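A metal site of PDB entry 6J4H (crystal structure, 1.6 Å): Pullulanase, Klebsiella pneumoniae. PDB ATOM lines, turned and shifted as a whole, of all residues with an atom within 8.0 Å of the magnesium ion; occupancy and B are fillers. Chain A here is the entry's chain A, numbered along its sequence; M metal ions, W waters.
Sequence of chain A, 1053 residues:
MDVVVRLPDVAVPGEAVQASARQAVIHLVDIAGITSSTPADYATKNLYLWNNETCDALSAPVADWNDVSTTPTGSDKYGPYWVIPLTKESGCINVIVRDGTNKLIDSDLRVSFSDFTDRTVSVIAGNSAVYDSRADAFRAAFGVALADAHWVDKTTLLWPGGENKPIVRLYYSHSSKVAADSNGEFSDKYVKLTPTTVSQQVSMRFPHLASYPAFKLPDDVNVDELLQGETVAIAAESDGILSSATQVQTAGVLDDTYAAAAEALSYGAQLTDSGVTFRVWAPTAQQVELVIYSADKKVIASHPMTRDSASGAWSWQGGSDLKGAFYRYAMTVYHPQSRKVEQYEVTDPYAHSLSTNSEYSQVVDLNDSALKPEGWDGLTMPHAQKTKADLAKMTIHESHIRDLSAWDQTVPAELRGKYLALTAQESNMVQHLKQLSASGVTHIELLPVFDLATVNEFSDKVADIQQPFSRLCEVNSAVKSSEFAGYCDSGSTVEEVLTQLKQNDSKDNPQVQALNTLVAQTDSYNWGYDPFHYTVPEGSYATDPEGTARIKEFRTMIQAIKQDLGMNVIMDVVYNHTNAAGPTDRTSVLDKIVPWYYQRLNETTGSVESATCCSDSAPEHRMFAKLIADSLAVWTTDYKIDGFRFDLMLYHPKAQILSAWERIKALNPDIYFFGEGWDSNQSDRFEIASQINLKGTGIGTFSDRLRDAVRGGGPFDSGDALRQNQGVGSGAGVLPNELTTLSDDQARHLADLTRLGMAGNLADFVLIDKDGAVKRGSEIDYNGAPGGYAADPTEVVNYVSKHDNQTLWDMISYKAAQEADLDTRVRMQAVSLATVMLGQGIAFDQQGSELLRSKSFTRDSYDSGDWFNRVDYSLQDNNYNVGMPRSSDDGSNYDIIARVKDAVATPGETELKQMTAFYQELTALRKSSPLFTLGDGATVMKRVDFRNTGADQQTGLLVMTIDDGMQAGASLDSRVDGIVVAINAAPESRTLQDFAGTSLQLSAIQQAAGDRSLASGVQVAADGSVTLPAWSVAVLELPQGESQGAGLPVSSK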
ATOM      1  N   SER A 929      -1.816  25.282   4.306  1.00  0.00           N
ATOM      2  CA  SER A 929      -3.152  25.187   4.871  1.00  0.00           C
ATOM      3  C   SER A 929      -3.301  26.094   6.081  1.00  0.00           C
ATOM      4  O   SER A 929      -2.405  26.148   6.935  1.00  0.00           O
ATOM      5  CB  SER A 929      -3.490  23.747   5.282  1.00  0.00           C
ATOM      6  OG  SER A 929      -4.744  23.672   5.942  1.00  0.00           O
ATOM      7  N   PRO A 930      -4.433  26.804   6.200  1.00  0.00           N
ATOM      8  CA  PRO A 930      -4.686  27.584   7.426  1.00  0.00           C
ATOM      9  C   PRO A 930      -4.879  26.731   8.678  1.00  0.00           C
ATOM     10  O   PRO A 930      -4.873  27.284   9.786  1.00  0.00           O
ATOM     11  CB  PRO A 930      -5.974  28.348   7.081  1.00  0.00           C
ATOM     12  CG  PRO A 930      -6.681  27.458   6.104  1.00  0.00           C
ATOM     13  CD  PRO A 930      -5.560  26.868   5.254  1.00  0.00           C
ATOM     14  N   LEU A 931      -5.042  25.407   8.552  1.00  0.00           N
ATOM     15  CA  LEU A 931      -5.189  24.551   9.721  1.00  0.00           C
ATOM     16  C   LEU A 931      -3.921  24.461  10.560  1.00  0.00           C
ATOM     17  O   LEU A 931      -4.015  24.190  11.768  1.00  0.00           O
ATOM     18  CB  LEU A 931      -5.643  23.153   9.287  1.00  0.00           C
ATOM     19  CG  LEU A 931      -7.024  23.128   8.621  1.00  0.00           C
ATOM     20  CD1 LEU A 931      -7.306  21.742   8.035  1.00  0.00           C
ATOM     21  CD2 LEU A 931      -8.095  23.524   9.621  1.00  0.00           C
ATOM     22  N   ARG A 943     -10.022  22.199  17.795  1.00  0.00           N
ATOM     23  CA  ARG A 943      -9.619  21.481  16.590  1.00  0.00           C
ATOM     24  C   ARG A 943      -8.423  20.554  16.760  1.00  0.00           C
ATOM     25  O   ARG A 943      -8.324  19.578  15.999  1.00  0.00           O
ATOM     26  CB  ARG A 943      -9.306  22.470  15.453  1.00  0.00           C
ATOM     27  CG  ARG A 943     -10.537  23.245  14.962  1.00  0.00           C
ATOM     28  CD  ARG A 943     -10.191  24.266  13.892  1.00  0.00           C
ATOM     29  NE  ARG A 943     -11.386  25.027  13.474  1.00  0.00           N
ATOM     30  CZ  ARG A 943     -12.018  24.868  12.304  1.00  0.00           C
ATOM     31  NH1 ARG A 943     -11.598  23.956  11.431  1.00  0.00           N
ATOM     32  NH2 ARG A 943     -13.063  25.630  12.015  1.00  0.00           N
ATOM     33  N   ASP A 963      -8.678  19.285  13.169  1.00  0.00           N
ATOM     34  CA  ASP A 963     -10.008  19.052  12.641  1.00  0.00           C
ATOM     35  C   ASP A 963     -10.464  20.195  11.726  1.00  0.00           C
ATOM     36  O   ASP A 963     -10.309  21.377  12.081  1.00  0.00           O
ATOM     37  CB  ASP A 963     -10.997  18.895  13.799  1.00  0.00           C
ATOM     38  CG  ASP A 963     -12.344  18.364  13.368  1.00  0.00           C
ATOM     39  OD1 ASP A 963     -12.441  17.788  12.259  1.00  0.00           O
ATOM     40  OD2 ASP A 963     -13.315  18.526  14.143  1.00  0.00           O
ATOM     41  N   ASP A 964     -11.031  19.862  10.560  1.00  0.00           N
ATOM     42  CA  ASP A 964     -11.761  20.816   9.737  1.00  0.00           C
ATOM     43  C   ASP A 964     -13.184  20.328   9.450  1.00  0.00           C
ATOM     44  O   ASP A 964     -13.832  20.842   8.537  1.00  0.00           O
ATOM     45  CB  ASP A 964     -11.042  21.095   8.414  1.00  0.00           C
ATOM     46  CG  ASP A 964     -11.380  22.483   7.838  1.00  0.00           C
ATOM     47  OD1 ASP A 964     -11.550  23.429   8.644  1.00  0.00           O
ATOM     48  OD2 ASP A 964     -11.456  22.634   6.601  1.00  0.00           O
ATOM     49  N   GLY A 965     -13.654  19.342  10.212  1.00  0.00           N
ATOM     50  CA  GLY A 965     -14.956  18.756  10.004  1.00  0.00           C
ATOM     51  C   GLY A 965     -16.068  19.503  10.728  1.00  0.00           C
ATOM     52  O   GLY A 965     -15.854  20.525  11.378  1.00  0.00           O
ATOM     53  N   ALA A 970     -16.804  26.021  10.923  1.00  0.00           N
ATOM     54  CA  ALA A 970     -16.675  26.209   9.485  1.00  0.00           C
ATOM     55  C   ALA A 970     -15.446  25.481   8.950  1.00  0.00           C
ATOM     56  O   ALA A 970     -14.451  25.282   9.650  1.00  0.00           O
ATOM     57  CB  ALA A 970     -16.584  27.692   9.145  1.00  0.00           C
ATOM     58  N   SER A 971     -15.525  25.078   7.685  1.00  0.00           N
ATOM     59  CA  SER A 971     -14.349  24.590   6.983  1.00  0.00           C
ATOM     60  C   SER A 971     -13.447  25.776   6.659  1.00  0.00           C
ATOM     61  O   SER A 971     -13.867  26.711   5.958  1.00  0.00           O
ATOM     62  CB  SER A 971     -14.759  23.844   5.700  1.00  0.00           C
ATOM     63  OG  SER A 971     -13.648  23.601   4.825  1.00  0.00           O
ATOM     64  N   LEU A 972     -12.231  25.764   7.206  1.00  0.00           N
ATOM     65  CA  LEU A 972     -11.255  26.806   6.906  1.00  0.00           C
ATOM     66  C   LEU A 972     -10.457  26.507   5.648  1.00  0.00           C
ATOM     67  O   LEU A 972      -9.844  27.422   5.084  1.00  0.00           O
ATOM     68  CB  LEU A 972     -10.298  26.988   8.094  1.00  0.00           C
ATOM     69  CG  LEU A 972     -10.969  27.263   9.444  1.00  0.00           C
ATOM     70  CD1 LEU A 972      -9.958  27.252  10.586  1.00  0.00           C
ATOM     71  CD2 LEU A 972     -11.731  28.588   9.407  1.00  0.00           C
ATOM     72  N   ASP A 973     -10.454  25.257   5.199  1.00  0.00           N
ATOM     73  CA  ASP A 973      -9.673  24.806   4.068  1.00  0.00           C
ATOM     74  C   ASP A 973     -10.600  24.012   3.160  1.00  0.00           C
ATOM     75  O   ASP A 973     -11.105  22.961   3.566  1.00  0.00           O
ATOM     76  CB  ASP A 973      -8.498  23.946   4.546  1.00  0.00           C
ATOM     77  CG  ASP A 973      -7.480  23.650   3.463  1.00  0.00           C
ATOM     78  OD1 ASP A 973      -7.813  23.680   2.256  1.00  0.00           O
ATOM     79  OD2 ASP A 973      -6.316  23.367   3.839  1.00  0.00           O
ATOM     80  N   SER A 974     -10.836  24.505   1.942  1.00  0.00           N
ATOM     81  CA  SER A 974     -11.808  23.833   1.073  1.00  0.00           C
ATOM     82  C   SER A 974     -11.292  22.513   0.531  1.00  0.00           C
ATOM     83  O   SER A 974     -12.084  21.695   0.042  1.00  0.00           O
ATOM     84  CB  SER A 974     -12.187  24.740  -0.103  1.00  0.00           C
ATOM     85  OG  SER A 974     -11.084  25.000  -0.940  1.00  0.00           O
ATOM     86  N   ARG A 975      -9.986  22.273   0.630  1.00  0.00           N
ATOM     87  CA  ARG A 975      -9.414  21.058   0.061  1.00  0.00           C
ATOM     88  C   ARG A 975      -9.433  19.878   1.023  1.00  0.00           C
ATOM     89  O   ARG A 975      -9.349  18.733   0.553  1.00  0.00           O
ATOM     90  CB  ARG A 975      -7.987  21.325  -0.389  1.00  0.00           C
ATOM     91  CG  ARG A 975      -7.873  22.412  -1.463  1.00  0.00           C
ATOM     92  CD  ARG A 975      -6.484  22.423  -2.107  1.00  0.00           C
ATOM     93  NE  ARG A 975      -6.354  23.482  -3.114  1.00  0.00           N
ATOM     94  CZ  ARG A 975      -5.291  23.654  -3.897  1.00  0.00           C
ATOM     95  NH1 ARG A 975      -5.268  24.636  -4.781  1.00  0.00           N
ATOM     96  NH2 ARG A 975      -4.241  22.838  -3.789  1.00  0.00           N
ATOM     97  N   VAL A 976      -9.518  20.106   2.335  1.00  0.00           N
ATOM     98  CA  VAL A 976      -9.398  19.015   3.312  1.00  0.00           C
ATOM     99  C   VAL A 976     -10.427  19.174   4.429  1.00  0.00           C
ATOM    100  O   VAL A 976     -10.828  20.299   4.777  1.00  0.00           O
ATOM    101  CB  VAL A 976      -7.979  18.932   3.931  1.00  0.00           C
ATOM    102  CG1 VAL A 976      -6.899  18.773   2.873  1.00  0.00           C
ATOM    103  CG2 VAL A 976      -7.701  20.144   4.815  1.00  0.00           C
ATOM    104  N   ASP A 977     -10.803  18.036   5.005  1.00  0.00           N
ATOM    105  CA  ASP A 977     -11.622  17.944   6.210  1.00  0.00           C
ATOM    106  C   ASP A 977     -10.803  17.730   7.475  1.00  0.00           C
ATOM    107  O   ASP A 977     -11.377  17.683   8.574  1.00  0.00           O
ATOM    108  CB  ASP A 977     -12.631  16.789   6.078  1.00  0.00           C
ATOM    109  CG  ASP A 977     -13.817  17.127   5.185  1.00  0.00           C
ATOM    110  OD1 ASP A 977     -14.284  18.280   5.190  1.00  0.00           O
ATOM    111  OD2 ASP A 977     -14.274  16.196   4.486  1.00  0.00           O
ATOM    112  N   GLY A 978      -9.496  17.569   7.352  1.00  0.00           N
ATOM    113  CA  GLY A 978      -8.654  17.339   8.518  1.00  0.00           C
ATOM    114  C   GLY A 978      -7.237  17.046   8.062  1.00  0.00           C
ATOM    115  O   GLY A 978      -7.009  16.635   6.930  1.00  0.00           O
ATOM    116  N   LEU A1038      -7.488  14.348   5.071  1.00  0.00           N
ATOM    117  CA  LEU A1038      -8.769  13.819   4.625  1.00  0.00           C
ATOM    118  C   LEU A1038      -9.269  14.707   3.496  1.00  0.00           C
ATOM    119  O   LEU A1038      -9.589  15.877   3.725  1.00  0.00           O
ATOM    120  CB  LEU A1038      -9.777  13.814   5.777  1.00  0.00           C
ATOM    121  CG  LEU A1038      -9.482  12.927   6.995  1.00  0.00           C
ATOM    122  CD1 LEU A1038     -10.499  13.168   8.094  1.00  0.00           C
ATOM    123  CD2 LEU A1038      -9.423  11.443   6.620  1.00  0.00           C
ATOM    124  N   PRO A1039      -9.338  14.212   2.263  1.00  0.00           N
ATOM    125  CA  PRO A1039      -9.796  15.059   1.153  1.00  0.00           C
ATOM    126  C   PRO A1039     -11.247  15.457   1.336  1.00  0.00           C
ATOM    127  O   PRO A1039     -12.099  14.636   1.695  1.00  0.00           O
ATOM    128  CB  PRO A1039      -9.598  14.171  -0.078  1.00  0.00           C
ATOM    129  CG  PRO A1039      -9.673  12.778   0.461  1.00  0.00           C
ATOM    130  CD  PRO A1039      -9.015  12.843   1.814  1.00  0.00           C
ATOM    131  N   GLN A1040     -11.548  16.730   1.063  1.00  0.00           N
ATOM    132  CA  GLN A1040     -12.901  17.246   1.221  1.00  0.00           C
ATOM    133  C   GLN A1040     -13.695  17.027  -0.060  1.00  0.00           C
ATOM    134  O   GLN A1040     -13.204  17.302  -1.155  1.00  0.00           O
ATOM    135  CB  GLN A1040     -12.873  18.722   1.595  1.00  0.00           C
ATOM    136  CG  GLN A1040     -14.261  19.315   1.870  1.00  0.00           C
ATOM    137  CD  GLN A1040     -14.153  20.635   2.605  1.00  0.00           C
ATOM    138  OE1 GLN A1040     -13.128  20.906   3.249  1.00  0.00           O
ATOM    139  NE2 GLN A1040     -15.195  21.459   2.516  1.00  0.00           N
ATOM    140  N   GLY A1041     -14.932  16.558   0.105  1.00  0.00           N
ATOM    141  CA  GLY A1041     -15.852  16.274  -0.975  1.00  0.00           C
ATOM    142  C   GLY A1041     -16.817  17.409  -1.215  1.00  0.00           C
ATOM    143  O   GLY A1041     -16.504  18.588  -0.990  1.00  0.00           O
ATOM    144  N   SER A1043     -19.519  18.378   0.259  1.00  0.00           N
ATOM    145  CA  SER A1043     -19.804  19.151   1.460  1.00  0.00           C
ATOM    146  C   SER A1043     -18.789  18.803   2.547  1.00  0.00           C
ATOM    147  O   SER A1043     -18.116  17.771   2.492  1.00  0.00           O
ATOM    148  CB  SER A1043     -21.231  18.920   1.975  1.00  0.00           C
ATOM    149  OG  SER A1043     -21.424  17.576   2.369  1.00  0.00           O
ATOM    150  N   GLN A1044     -18.685  19.702   3.522  1.00  0.00           N
ATOM    151  CA  GLN A1044     -17.825  19.464   4.683  1.00  0.00           C
ATOM    152  C   GLN A1044     -18.120  18.113   5.307  1.00  0.00           C
ATOM    153  O   GLN A1044     -19.285  17.744   5.513  1.00  0.00           O
ATOM    154  CB  GLN A1044     -18.039  20.583   5.696  1.00  0.00           C
ATOM    155  CG  GLN A1044     -17.203  20.472   6.965  1.00  0.00           C
ATOM    156  CD  GLN A1044     -17.515  21.569   7.948  1.00  0.00           C
ATOM    157  OE1 GLN A1044     -18.659  22.039   8.033  1.00  0.00           O
ATOM    158  NE2 GLN A1044     -16.522  21.983   8.722  1.00  0.00           N
ATOM    159  N   GLY A1045     -17.053  17.364   5.611  1.00  0.00           N
ATOM    160  CA  GLY A1045     -17.173  16.024   6.143  1.00  0.00           C
ATOM    161  C   GLY A1045     -17.033  15.966   7.661  1.00  0.00           C
ATOM    162  O   GLY A1045     -17.028  16.979   8.359  1.00  0.00           O
HETATM  163 MG    MG M   1     -12.222  21.904   4.815  1.00  0.00          MG
HETATM  164  O   HOH W   1     -13.611  20.767   5.833  1.00  0.00           O
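The magnesium ion is bound by O of Asp 973 (2.0 Å), water W1 (2.1 Å), OE1 of Gln 1040 (2.1 Å), OD2 of Asp 964 (2.1 Å), O of Val 976 (2.1 Å) and OG of Ser 971 (2.2 Å).
The side-chain hydroxyl of Ser 929 lies within hydrogen-bond range of the side-chain carboxylate of Asp 973 (2.6 Å).
O of Ser 974 lies close to OE1 of Gln 1040.
The side-chain amide oxygen (OE1) of Gln 1040 lies close to the side-chain carboxylate (OD1) of Asp 977, 3.5 Å away.
The backbone carbonyl oxygen (O) of Arg 975 is in hydrogen-bond range of the backbone NH (N) of Gln 1040 (3.0 Å).
The backbone NH (N) of Leu 972 sits at hydrogen-bond distance from the side-chain carboxylate (OD1) of Asp 964 (2.8 Å).
The backbone carbonyl oxygen (O) of Asp 964 sits at hydrogen-bond distance from the side-chain amide nitrogen (NE2) of Gln 1044 (2.9 Å).
The guanidinium group (NH1) of Arg 943 is in salt-bridge range of the side-chain carboxylate (OD1) of Asp 964, 2.8 Å away.
The backbone NH (N) of Ser 971 lies close to the side-chain amide nitrogen (NE2) of Gln 1044 (3.4 Å).
Five residues have an atom within 4 Å of the magnesium ion: Asp 964, Ser 971, Asp 973, Val 976 and Gln 1040.
The nearest printed residue that does not touch the magnesium ion is Ser 974 (4.1 Å).
Water W1 lies within hydrogen-bond range of the side-chain carboxylate (OD1) of Asp 977 (2.7 Å) and the backbone carbonyl oxygen (O) of Asp 964 (2.7 Å).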
